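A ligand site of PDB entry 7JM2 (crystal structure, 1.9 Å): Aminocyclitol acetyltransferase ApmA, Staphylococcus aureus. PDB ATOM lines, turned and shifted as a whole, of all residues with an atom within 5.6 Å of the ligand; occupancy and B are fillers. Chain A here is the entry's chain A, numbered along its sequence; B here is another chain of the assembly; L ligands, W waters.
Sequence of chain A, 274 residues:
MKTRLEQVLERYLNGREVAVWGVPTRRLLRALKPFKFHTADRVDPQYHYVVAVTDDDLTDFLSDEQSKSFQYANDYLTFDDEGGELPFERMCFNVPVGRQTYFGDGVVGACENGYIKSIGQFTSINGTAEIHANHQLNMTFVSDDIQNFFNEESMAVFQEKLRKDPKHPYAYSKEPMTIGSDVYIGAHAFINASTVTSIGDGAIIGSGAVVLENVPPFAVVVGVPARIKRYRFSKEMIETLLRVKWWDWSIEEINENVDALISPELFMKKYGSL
A nitrogen (N1) of the ligand is in hydrogen-bond range of a ring nitrogen (NE2) of His 135.
N1 of the ligand sits at hydrogen-bond distance from OH of Tyr 102 of chain B (3.1 Å).
An oxygen (O8) of the ligand is in hydrogen-bond range of the side-chain amide oxygen (OE1) of Gln 147, at 2.6 Å.
The side-chain amide oxygen of Asn 113 is in hydrogen-bond range of an oxygen (O3) of the ligand, at 3.3 Å.
The side-chain carboxylate of Asp 145 lies within salt-bridge range of a nitrogen (N5) of the ligand, at 2.9 Å.
The side-chain amide nitrogen (NE2) of Gln 159 lies within hydrogen-bond range of an oxygen (O8) of the ligand.
A nitrogen (N5) of the ligand lies within salt-bridge range of the side-chain carboxylate (OD2) of Asp 144 (2.9 Å).
OE1 of Glu 85 of chain B is in salt-bridge range of N4 of the ligand (2.9 Å).
The side-chain amide nitrogen (NE2) of Gln 147 sits at hydrogen-bond distance from the backbone carbonyl oxygen (O) of Asp 144.
OH of Tyr 172 lies within hydrogen-bond range of OE1 of Gln 159 (2.6 Å).
The side-chain carboxylate (OD1) of Asp 144 lies within hydrogen-bond range of the side-chain hydroxyl (OH) of Tyr 102 of chain B (2.6 Å).
SD of Met 155 is in hydrogen-bond range of NE2 of Gln 159.
The side-chain hydroxyl of Tyr 102 of chain B lies close to the side-chain hydroxyl of Ser 124 of chain B (3.3 Å).
The side-chain hydroxyl (OG) of Ser 124 of chain B is in hydrogen-bond range of the side-chain carboxylate (OD1) of Asp 144 (3.3 Å).
Tyr 170 touches the ligand.
Tyr 172 touches the ligand.
Hydrophobic or aromatic side chains that line the ligand: His 135, Tyr 170, Tyr 172 and Tyr 102 of chain B.
Within 4 Å of the ligand: Asn 113, His 135, Asp 144, Asp 145, Gln 147, Gln 159, Tyr 170, Tyr 172, Glu 85 of chain B and Tyr 102 of chain B.
Water W11 bridges O9 of the ligand (2.6 Å) and O of Tyr 170 (2.9 Å).
Water W10 lies within hydrogen-bond range of OD1 of Asn 113 (2.7 Å) and N2 of the ligand (2.8 Å).
Water W5 lies within hydrogen-bond range of a nitrogen (N1) of the ligand (3.0 Å) and the side-chain hydroxyl (OH) of Tyr 184 of chain B (3.0 Å).
Water W8 lies within hydrogen-bond range of OH of Tyr 115 (2.5 Å), O6 of the ligand (3.0 Å) and O of Tyr 170 (3.4 Å).
Water W3 bridges the side-chain carboxylate (OD2) of Asp 144 and an oxygen (O4) of the ligand.
Water W15 lies within hydrogen-bond range of a nitrogen (N4) of the ligand (3.2 Å) and the side-chain carboxylate of Glu 85 of chain B (3.3 Å).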
ATOM      1  N   ASN A 113       9.762 -23.357 -21.393  1.00  0.00           N
ATOM      2  CA  ASN A 113      10.543 -22.629 -20.405  1.00  0.00           C
ATOM      3  C   ASN A 113      11.269 -23.535 -19.417  1.00  0.00           C
ATOM      4  O   ASN A 113      12.028 -23.014 -18.596  1.00  0.00           O
ATOM      5  CB  ASN A 113       9.641 -21.677 -19.619  1.00  0.00           C
ATOM      6  CG  ASN A 113       9.382 -20.416 -20.364  1.00  0.00           C
ATOM      7  OD1 ASN A 113      10.220 -19.981 -21.152  1.00  0.00           O
ATOM      8  ND2 ASN A 113       8.205 -19.814 -20.157  1.00  0.00           N
ATOM      9  N   TYR A 115       9.723 -25.278 -17.069  1.00  0.00           N
ATOM     10  CA  TYR A 115       9.039 -25.257 -15.786  1.00  0.00           C
ATOM     11  C   TYR A 115       8.380 -26.584 -15.436  1.00  0.00           C
ATOM     12  O   TYR A 115       7.908 -26.741 -14.306  1.00  0.00           O
ATOM     13  CB  TYR A 115       7.970 -24.156 -15.773  1.00  0.00           C
ATOM     14  CG  TYR A 115       8.506 -22.746 -15.902  1.00  0.00           C
ATOM     15  CD1 TYR A 115       9.825 -22.458 -15.611  1.00  0.00           C
ATOM     16  CD2 TYR A 115       7.680 -21.715 -16.342  1.00  0.00           C
ATOM     17  CE1 TYR A 115      10.316 -21.160 -15.733  1.00  0.00           C
ATOM     18  CE2 TYR A 115       8.160 -20.414 -16.471  1.00  0.00           C
ATOM     19  CZ  TYR A 115       9.476 -20.146 -16.162  1.00  0.00           C
ATOM     20  OH  TYR A 115       9.949 -18.863 -16.302  1.00  0.00           O
ATOM     21  N   HIS A 135       9.289 -13.304 -10.760  1.00  0.00           N
ATOM     22  CA  HIS A 135      10.541 -12.568 -10.885  1.00  0.00           C
ATOM     23  C   HIS A 135      11.267 -12.573  -9.538  1.00  0.00           C
ATOM     24  O   HIS A 135      10.743 -13.035  -8.519  1.00  0.00           O
ATOM     25  CB  HIS A 135      10.275 -11.138 -11.338  1.00  0.00           C
ATOM     26  CG  HIS A 135       9.805 -11.024 -12.747  1.00  0.00           C
ATOM     27  ND1 HIS A 135       9.866  -9.846 -13.471  1.00  0.00           N
ATOM     28  CD2 HIS A 135       9.230 -11.940 -13.573  1.00  0.00           C
ATOM     29  CE1 HIS A 135       9.372 -10.037 -14.670  1.00  0.00           C
ATOM     30  NE2 HIS A 135       8.980 -11.295 -14.765  1.00  0.00           N
ATOM     31  N   ASP A 144      12.492  -7.962 -15.198  1.00  0.00           N
ATOM     32  CA  ASP A 144      13.419  -8.897 -15.833  1.00  0.00           C
ATOM     33  C   ASP A 144      14.165  -8.248 -17.003  1.00  0.00           C
ATOM     34  O   ASP A 144      15.378  -8.404 -17.093  1.00  0.00           O
ATOM     35  CB  ASP A 144      12.683 -10.165 -16.310  1.00  0.00           C
ATOM     36  CG  ASP A 144      11.666  -9.907 -17.423  1.00  0.00           C
ATOM     37  OD1 ASP A 144      10.930  -8.905 -17.341  1.00  0.00           O
ATOM     38  OD2 ASP A 144      11.569 -10.731 -18.349  1.00  0.00           O
ATOM     39  N   ASP A 145      13.500  -7.494 -17.872  1.00  0.00           N
ATOM     40  CA  ASP A 145      14.179  -7.063 -19.092  1.00  0.00           C
ATOM     41  C   ASP A 145      15.131  -5.896 -18.874  1.00  0.00           C
ATOM     42  O   ASP A 145      15.833  -5.495 -19.815  1.00  0.00           O
ATOM     43  CB  ASP A 145      13.161  -6.753 -20.179  1.00  0.00           C
ATOM     44  CG  ASP A 145      12.636  -8.018 -20.843  1.00  0.00           C
ATOM     45  OD1 ASP A 145      13.336  -9.048 -20.728  1.00  0.00           O
ATOM     46  OD2 ASP A 145      11.546  -8.000 -21.437  1.00  0.00           O
ATOM     47  N   GLN A 147      17.687  -6.483 -17.483  1.00  0.00           N
ATOM     48  CA  GLN A 147      18.948  -7.197 -17.684  1.00  0.00           C
ATOM     49  C   GLN A 147      19.452  -7.122 -19.122  1.00  0.00           C
ATOM     50  O   GLN A 147      20.632  -7.398 -19.351  1.00  0.00           O
ATOM     51  CB  GLN A 147      18.810  -8.662 -17.280  1.00  0.00           C
ATOM     52  CG  GLN A 147      18.026  -9.505 -18.259  1.00  0.00           C
ATOM     53  CD  GLN A 147      17.705 -10.876 -17.683  1.00  0.00           C
ATOM     54  OE1 GLN A 147      18.427 -11.845 -17.943  1.00  0.00           O
ATOM     55  NE2 GLN A 147      16.650 -10.958 -16.888  1.00  0.00           N
ATOM     56  N   MET A 155      25.675  -8.576 -15.419  1.00  0.00           N
ATOM     57  CA  MET A 155      24.837  -9.761 -15.566  1.00  0.00           C
ATOM     58  C   MET A 155      25.330 -10.903 -14.685  1.00  0.00           C
ATOM     59  O   MET A 155      24.527 -11.715 -14.203  1.00  0.00           O
ATOM     60  CB  MET A 155      24.814 -10.188 -17.037  1.00  0.00           C
ATOM     61  CG  MET A 155      24.056 -11.477 -17.319  1.00  0.00           C
ATOM     62  SD  MET A 155      22.256 -11.323 -17.174  1.00  0.00           S
ATOM     63  CE  MET A 155      21.900 -10.319 -18.620  1.00  0.00           C
ATOM     64  N   PHE A 158      24.227 -10.357 -11.117  1.00  0.00           N
ATOM     65  CA  PHE A 158      22.770 -10.498 -11.086  1.00  0.00           C
ATOM     66  C   PHE A 158      22.379 -11.968 -11.160  1.00  0.00           C
ATOM     67  O   PHE A 158      21.581 -12.458 -10.353  1.00  0.00           O
ATOM     68  CB  PHE A 158      22.170  -9.700 -12.247  1.00  0.00           C
ATOM     69  CG  PHE A 158      20.718 -10.009 -12.527  1.00  0.00           C
ATOM     70  CD1 PHE A 158      19.727  -9.588 -11.665  1.00  0.00           C
ATOM     71  CD2 PHE A 158      20.356 -10.685 -13.692  1.00  0.00           C
ATOM     72  CE1 PHE A 158      18.386  -9.860 -11.930  1.00  0.00           C
ATOM     73  CE2 PHE A 158      19.026 -10.950 -13.968  1.00  0.00           C
ATOM     74  CZ  PHE A 158      18.044 -10.543 -13.088  1.00  0.00           C
ATOM     75  N   GLN A 159      22.955 -12.703 -12.116  1.00  0.00           N
ATOM     76  CA  GLN A 159      22.692 -14.128 -12.207  1.00  0.00           C
ATOM     77  C   GLN A 159      23.127 -14.847 -10.931  1.00  0.00           C
ATOM     78  O   GLN A 159      22.391 -15.703 -10.423  1.00  0.00           O
ATOM     79  CB  GLN A 159      23.383 -14.743 -13.425  1.00  0.00           C
ATOM     80  CG  GLN A 159      22.742 -14.345 -14.749  1.00  0.00           C
ATOM     81  CD  GLN A 159      21.355 -14.890 -14.919  1.00  0.00           C
ATOM     82  OE1 GLN A 159      21.045 -15.957 -14.399  1.00  0.00           O
ATOM     83  NE2 GLN A 159      20.492 -14.152 -15.626  1.00  0.00           N
ATOM     84  N   LEU A 162      20.610 -14.701  -8.299  1.00  0.00           N
ATOM     85  CA  LEU A 162      19.395 -15.452  -8.619  1.00  0.00           C
ATOM     86  C   LEU A 162      19.457 -16.901  -8.144  1.00  0.00           C
ATOM     87  O   LEU A 162      18.420 -17.455  -7.752  1.00  0.00           O
ATOM     88  CB  LEU A 162      19.119 -15.375 -10.124  1.00  0.00           C
ATOM     89  CG  LEU A 162      18.572 -14.070 -10.726  1.00  0.00           C
ATOM     90  CD1 LEU A 162      18.339 -14.185 -12.246  1.00  0.00           C
ATOM     91  CD2 LEU A 162      17.299 -13.593 -10.037  1.00  0.00           C
ATOM     92  N   TYR A 170      12.261 -17.115 -11.459  1.00  0.00           N
ATOM     93  CA  TYR A 170      12.329 -17.745 -12.790  1.00  0.00           C
ATOM     94  C   TYR A 170      12.506 -19.267 -12.707  1.00  0.00           C
ATOM     95  O   TYR A 170      13.039 -19.885 -13.635  1.00  0.00           O
ATOM     96  CB  TYR A 170      13.450 -17.126 -13.627  1.00  0.00           C
ATOM     97  CG  TYR A 170      13.435 -15.620 -13.565  1.00  0.00           C
ATOM     98  CD1 TYR A 170      12.434 -14.892 -14.199  1.00  0.00           C
ATOM     99  CD2 TYR A 170      14.381 -14.925 -12.830  1.00  0.00           C
ATOM    100  CE1 TYR A 170      12.402 -13.507 -14.135  1.00  0.00           C
ATOM    101  CE2 TYR A 170      14.351 -13.541 -12.757  1.00  0.00           C
ATOM    102  CZ  TYR A 170      13.370 -12.840 -13.406  1.00  0.00           C
ATOM    103  OH  TYR A 170      13.349 -11.459 -13.335  1.00  0.00           O
ATOM    104  N   TYR A 172      14.549 -20.863 -10.890  1.00  0.00           N
ATOM    105  CA  TYR A 172      15.910 -21.281 -10.611  1.00  0.00           C
ATOM    106  C   TYR A 172      15.928 -22.159  -9.363  1.00  0.00           C
ATOM    107  O   TYR A 172      15.097 -22.022  -8.473  1.00  0.00           O
ATOM    108  CB  TYR A 172      16.816 -20.080 -10.362  1.00  0.00           C
ATOM    109  CG  TYR A 172      17.300 -19.324 -11.571  1.00  0.00           C
ATOM    110  CD1 TYR A 172      16.619 -19.360 -12.786  1.00  0.00           C
ATOM    111  CD2 TYR A 172      18.455 -18.554 -11.483  1.00  0.00           C
ATOM    112  CE1 TYR A 172      17.090 -18.646 -13.884  1.00  0.00           C
ATOM    113  CE2 TYR A 172      18.920 -17.840 -12.560  1.00  0.00           C
ATOM    114  CZ  TYR A 172      18.238 -17.886 -13.756  1.00  0.00           C
ATOM    115  OH  TYR A 172      18.747 -17.156 -14.798  1.00  0.00           O
ATOM    116  N   ASP B  81       3.418  -7.511 -32.521  1.00  0.00           N
ATOM    117  CA  ASP B  81       3.977  -7.473 -31.174  1.00  0.00           C
ATOM    118  C   ASP B  81       3.962  -6.038 -30.661  1.00  0.00           C
ATOM    119  O   ASP B  81       4.957  -5.528 -30.145  1.00  0.00           O
ATOM    120  CB  ASP B  81       5.394  -8.056 -31.165  1.00  0.00           C
ATOM    121  CG  ASP B  81       5.952  -8.251 -29.778  1.00  0.00           C
ATOM    122  OD1 ASP B  81       5.174  -8.440 -28.804  1.00  0.00           O
ATOM    123  OD2 ASP B  81       7.198  -8.195 -29.650  1.00  0.00           O
ATOM    124  N   GLY B  84       5.503  -5.270 -27.401  1.00  0.00           N
ATOM    125  CA  GLY B  84       6.813  -5.820 -27.116  1.00  0.00           C
ATOM    126  C   GLY B  84       7.815  -4.785 -26.644  1.00  0.00           C
ATOM    127  O   GLY B  84       7.754  -3.604 -27.011  1.00  0.00           O
ATOM    128  N   GLU B  85       8.781  -5.245 -25.857  1.00  0.00           N
ATOM    129  CA  GLU B  85       9.779  -4.383 -25.237  1.00  0.00           C
ATOM    130  C   GLU B  85      10.767  -3.859 -26.275  1.00  0.00           C
ATOM    131  O   GLU B  85      11.032  -4.503 -27.284  1.00  0.00           O
ATOM    132  CB  GLU B  85      10.528  -5.142 -24.148  1.00  0.00           C
ATOM    133  CG  GLU B  85      11.501  -6.213 -24.651  1.00  0.00           C
ATOM    134  CD  GLU B  85      10.838  -7.565 -24.944  1.00  0.00           C
ATOM    135  OE1 GLU B  85       9.586  -7.656 -24.932  1.00  0.00           O
ATOM    136  OE2 GLU B  85      11.584  -8.542 -25.177  1.00  0.00           O
ATOM    137  N   TYR B 102       7.006  -4.222 -21.463  1.00  0.00           N
ATOM    138  CA  TYR B 102       6.203  -5.063 -22.327  1.00  0.00           C
ATOM    139  C   TYR B 102       4.812  -5.301 -21.746  1.00  0.00           C
ATOM    140  O   TYR B 102       4.608  -5.306 -20.523  1.00  0.00           O
ATOM    141  CB  TYR B 102       6.866  -6.423 -22.582  1.00  0.00           C
ATOM    142  CG  TYR B 102       7.283  -7.207 -21.350  1.00  0.00           C
ATOM    143  CD1 TYR B 102       6.411  -8.087 -20.731  1.00  0.00           C
ATOM    144  CD2 TYR B 102       8.579  -7.068 -20.826  1.00  0.00           C
ATOM    145  CE1 TYR B 102       6.808  -8.818 -19.633  1.00  0.00           C
ATOM    146  CE2 TYR B 102       8.969  -7.786 -19.725  1.00  0.00           C
ATOM    147  CZ  TYR B 102       8.080  -8.670 -19.134  1.00  0.00           C
ATOM    148  OH  TYR B 102       8.467  -9.397 -18.044  1.00  0.00           O
ATOM    149  N   SER B 124       6.640  -4.836 -16.434  1.00  0.00           N
ATOM    150  CA  SER B 124       6.459  -6.187 -16.938  1.00  0.00           C
ATOM    151  C   SER B 124       5.010  -6.611 -16.742  1.00  0.00           C
ATOM    152  O   SER B 124       4.585  -6.888 -15.620  1.00  0.00           O
ATOM    153  CB  SER B 124       7.402  -7.171 -16.248  1.00  0.00           C
ATOM    154  OG  SER B 124       8.736  -6.657 -16.193  1.00  0.00           O
ATOM    155  N   TYR B 184       5.071  -4.862 -11.918  1.00  0.00           N
ATOM    156  CA  TYR B 184       4.799  -6.217 -12.387  1.00  0.00           C
ATOM    157  C   TYR B 184       3.302  -6.484 -12.311  1.00  0.00           C
ATOM    158  O   TYR B 184       2.671  -6.196 -11.296  1.00  0.00           O
ATOM    159  CB  TYR B 184       5.554  -7.272 -11.561  1.00  0.00           C
ATOM    160  CG  TYR B 184       5.281  -8.712 -12.007  1.00  0.00           C
ATOM    161  CD1 TYR B 184       4.183  -9.419 -11.518  1.00  0.00           C
ATOM    162  CD2 TYR B 184       6.112  -9.353 -12.905  1.00  0.00           C
ATOM    163  CE1 TYR B 184       3.923 -10.737 -11.935  1.00  0.00           C
ATOM    164  CE2 TYR B 184       5.870 -10.646 -13.322  1.00  0.00           C
ATOM    165  CZ  TYR B 184       4.778 -11.334 -12.832  1.00  0.00           C
ATOM    166  OH  TYR B 184       4.556 -12.622 -13.262  1.00  0.00           O
HETATM  167  C1  LIG L   1       8.138 -13.381 -19.330  1.00  0.00           C
HETATM  168  C2  LIG L   1       8.342 -13.468 -17.794  1.00  0.00           C
HETATM  169  C3  LIG L   1       9.808 -13.568 -17.381  1.00  0.00           C
HETATM  170  C4  LIG L   1      10.527 -14.653 -18.129  1.00  0.00           C
HETATM  171  C5  LIG L   1      10.318 -14.511 -19.669  1.00  0.00           C
HETATM  172  C6  LIG L   1      11.059 -15.549 -20.436  1.00  0.00           C
HETATM  173  C7  LIG L   1      12.562 -15.503 -20.066  1.00  0.00           C
HETATM  174  C8  LIG L   1      12.829 -15.620 -18.544  1.00  0.00           C
HETATM  175  C9  LIG L   1      13.143 -16.357 -22.245  1.00  0.00           C
HETATM  176  O1  LIG L   1       8.865 -14.523 -20.003  1.00  0.00           O
HETATM  177  O2  LIG L   1      11.981 -14.652 -17.776  1.00  0.00           O
HETATM  178  N1  LIG L   1       7.786 -12.282 -17.196  1.00  0.00           N
HETATM  179  N2  LIG L   1      13.302 -16.542 -20.783  1.00  0.00           N
HETATM  180  O3  LIG L   1      10.540 -16.837 -20.086  1.00  0.00           O
HETATM  181  O4  LIG L   1      14.134 -15.303 -18.320  1.00  0.00           O
HETATM  182  O5  LIG L   1       8.568 -12.153 -19.825  1.00  0.00           O
HETATM  183  C10 LIG L   1      14.605 -15.788 -17.129  1.00  0.00           C
HETATM  184  C11 LIG L   1      15.752 -14.905 -16.653  1.00  0.00           C
HETATM  185  C12 LIG L   1      16.941 -15.009 -17.559  1.00  0.00           C
HETATM  186  C13 LIG L   1      17.368 -16.442 -17.763  1.00  0.00           C
HETATM  187  C14 LIG L   1      16.195 -17.307 -18.233  1.00  0.00           C
HETATM  188  C15 LIG L   1      16.594 -18.745 -18.351  1.00  0.00           C
HETATM  189  O6  LIG L   1      15.052 -17.207 -17.304  1.00  0.00           O
HETATM  190  N3  LIG L   1      18.469 -16.524 -18.774  1.00  0.00           N
HETATM  191  O7  LIG L   1      15.253 -13.568 -16.610  1.00  0.00           O
HETATM  192  O8  LIG L   1      18.072 -14.261 -17.002  1.00  0.00           O
HETATM  193  O9  LIG L   1      16.594 -19.343 -17.094  1.00  0.00           O
HETATM  194  C16 LIG L   1       8.550 -12.004 -21.273  1.00  0.00           C
HETATM  195  C17 LIG L   1       7.157 -11.867 -21.867  1.00  0.00           C
HETATM  196  C18 LIG L   1       7.228 -11.596 -23.380  1.00  0.00           C
HETATM  197  C19 LIG L   1       8.014 -10.291 -23.701  1.00  0.00           C
HETATM  198  C20 LIG L   1       9.402 -10.353 -23.089  1.00  0.00           C
HETATM  199  C21 LIG L   1       9.348 -10.692 -21.595  1.00  0.00           C
HETATM  200  N4  LIG L   1       8.123 -10.129 -25.169  1.00  0.00           N
HETATM  201  N5  LIG L   1      10.703 -10.792 -21.093  1.00  0.00           N
HETATM  202  O10 LIG L   1       6.404 -13.051 -21.683  1.00  0.00           O
HETATM  203  O11 LIG L   1       5.935 -11.463 -23.889  1.00  0.00           O
HETATM  204  O   HOH W   1       5.879  -9.395 -26.180  1.00  0.00           O
HETATM  205  O   HOH W   2       9.432 -12.490 -26.082  1.00  0.00           O
HETATM  206  O   HOH W   3      13.803 -12.260 -19.141  1.00  0.00           O
HETATM  207  O   HOH W   4       4.824 -12.491 -17.791  1.00  0.00           O
HETATM  208  O   HOH W   5       6.677 -13.993 -14.957  1.00  0.00           O
HETATM  209  O   HOH W   6      16.297 -15.648 -21.523  1.00  0.00           O
HETATM  210  O   HOH W   7      11.993 -12.773 -22.394  1.00  0.00           O
HETATM  211  O   HOH W   8      12.375 -18.493 -16.704  1.00  0.00           O
HETATM  212  O   HOH W   9       2.860 -10.419 -24.908  1.00  0.00           O
HETATM  213  O   HOH W  10      12.448 -19.061 -19.831  1.00  0.00           O
HETATM  214  O   HOH W  11      14.258 -20.159 -16.271  1.00  0.00           O
HETATM  215  O   HOH W  12       3.598 -12.553 -20.741  1.00  0.00           O
HETATM  216  O   HOH W  13       7.489 -15.240 -22.990  1.00  0.00           O
HETATM  217  O   HOH W  14       7.666 -16.991 -20.924  1.00  0.00           O
HETATM  218  O   HOH W  15       8.978  -8.891 -27.960  1.00  0.00           O
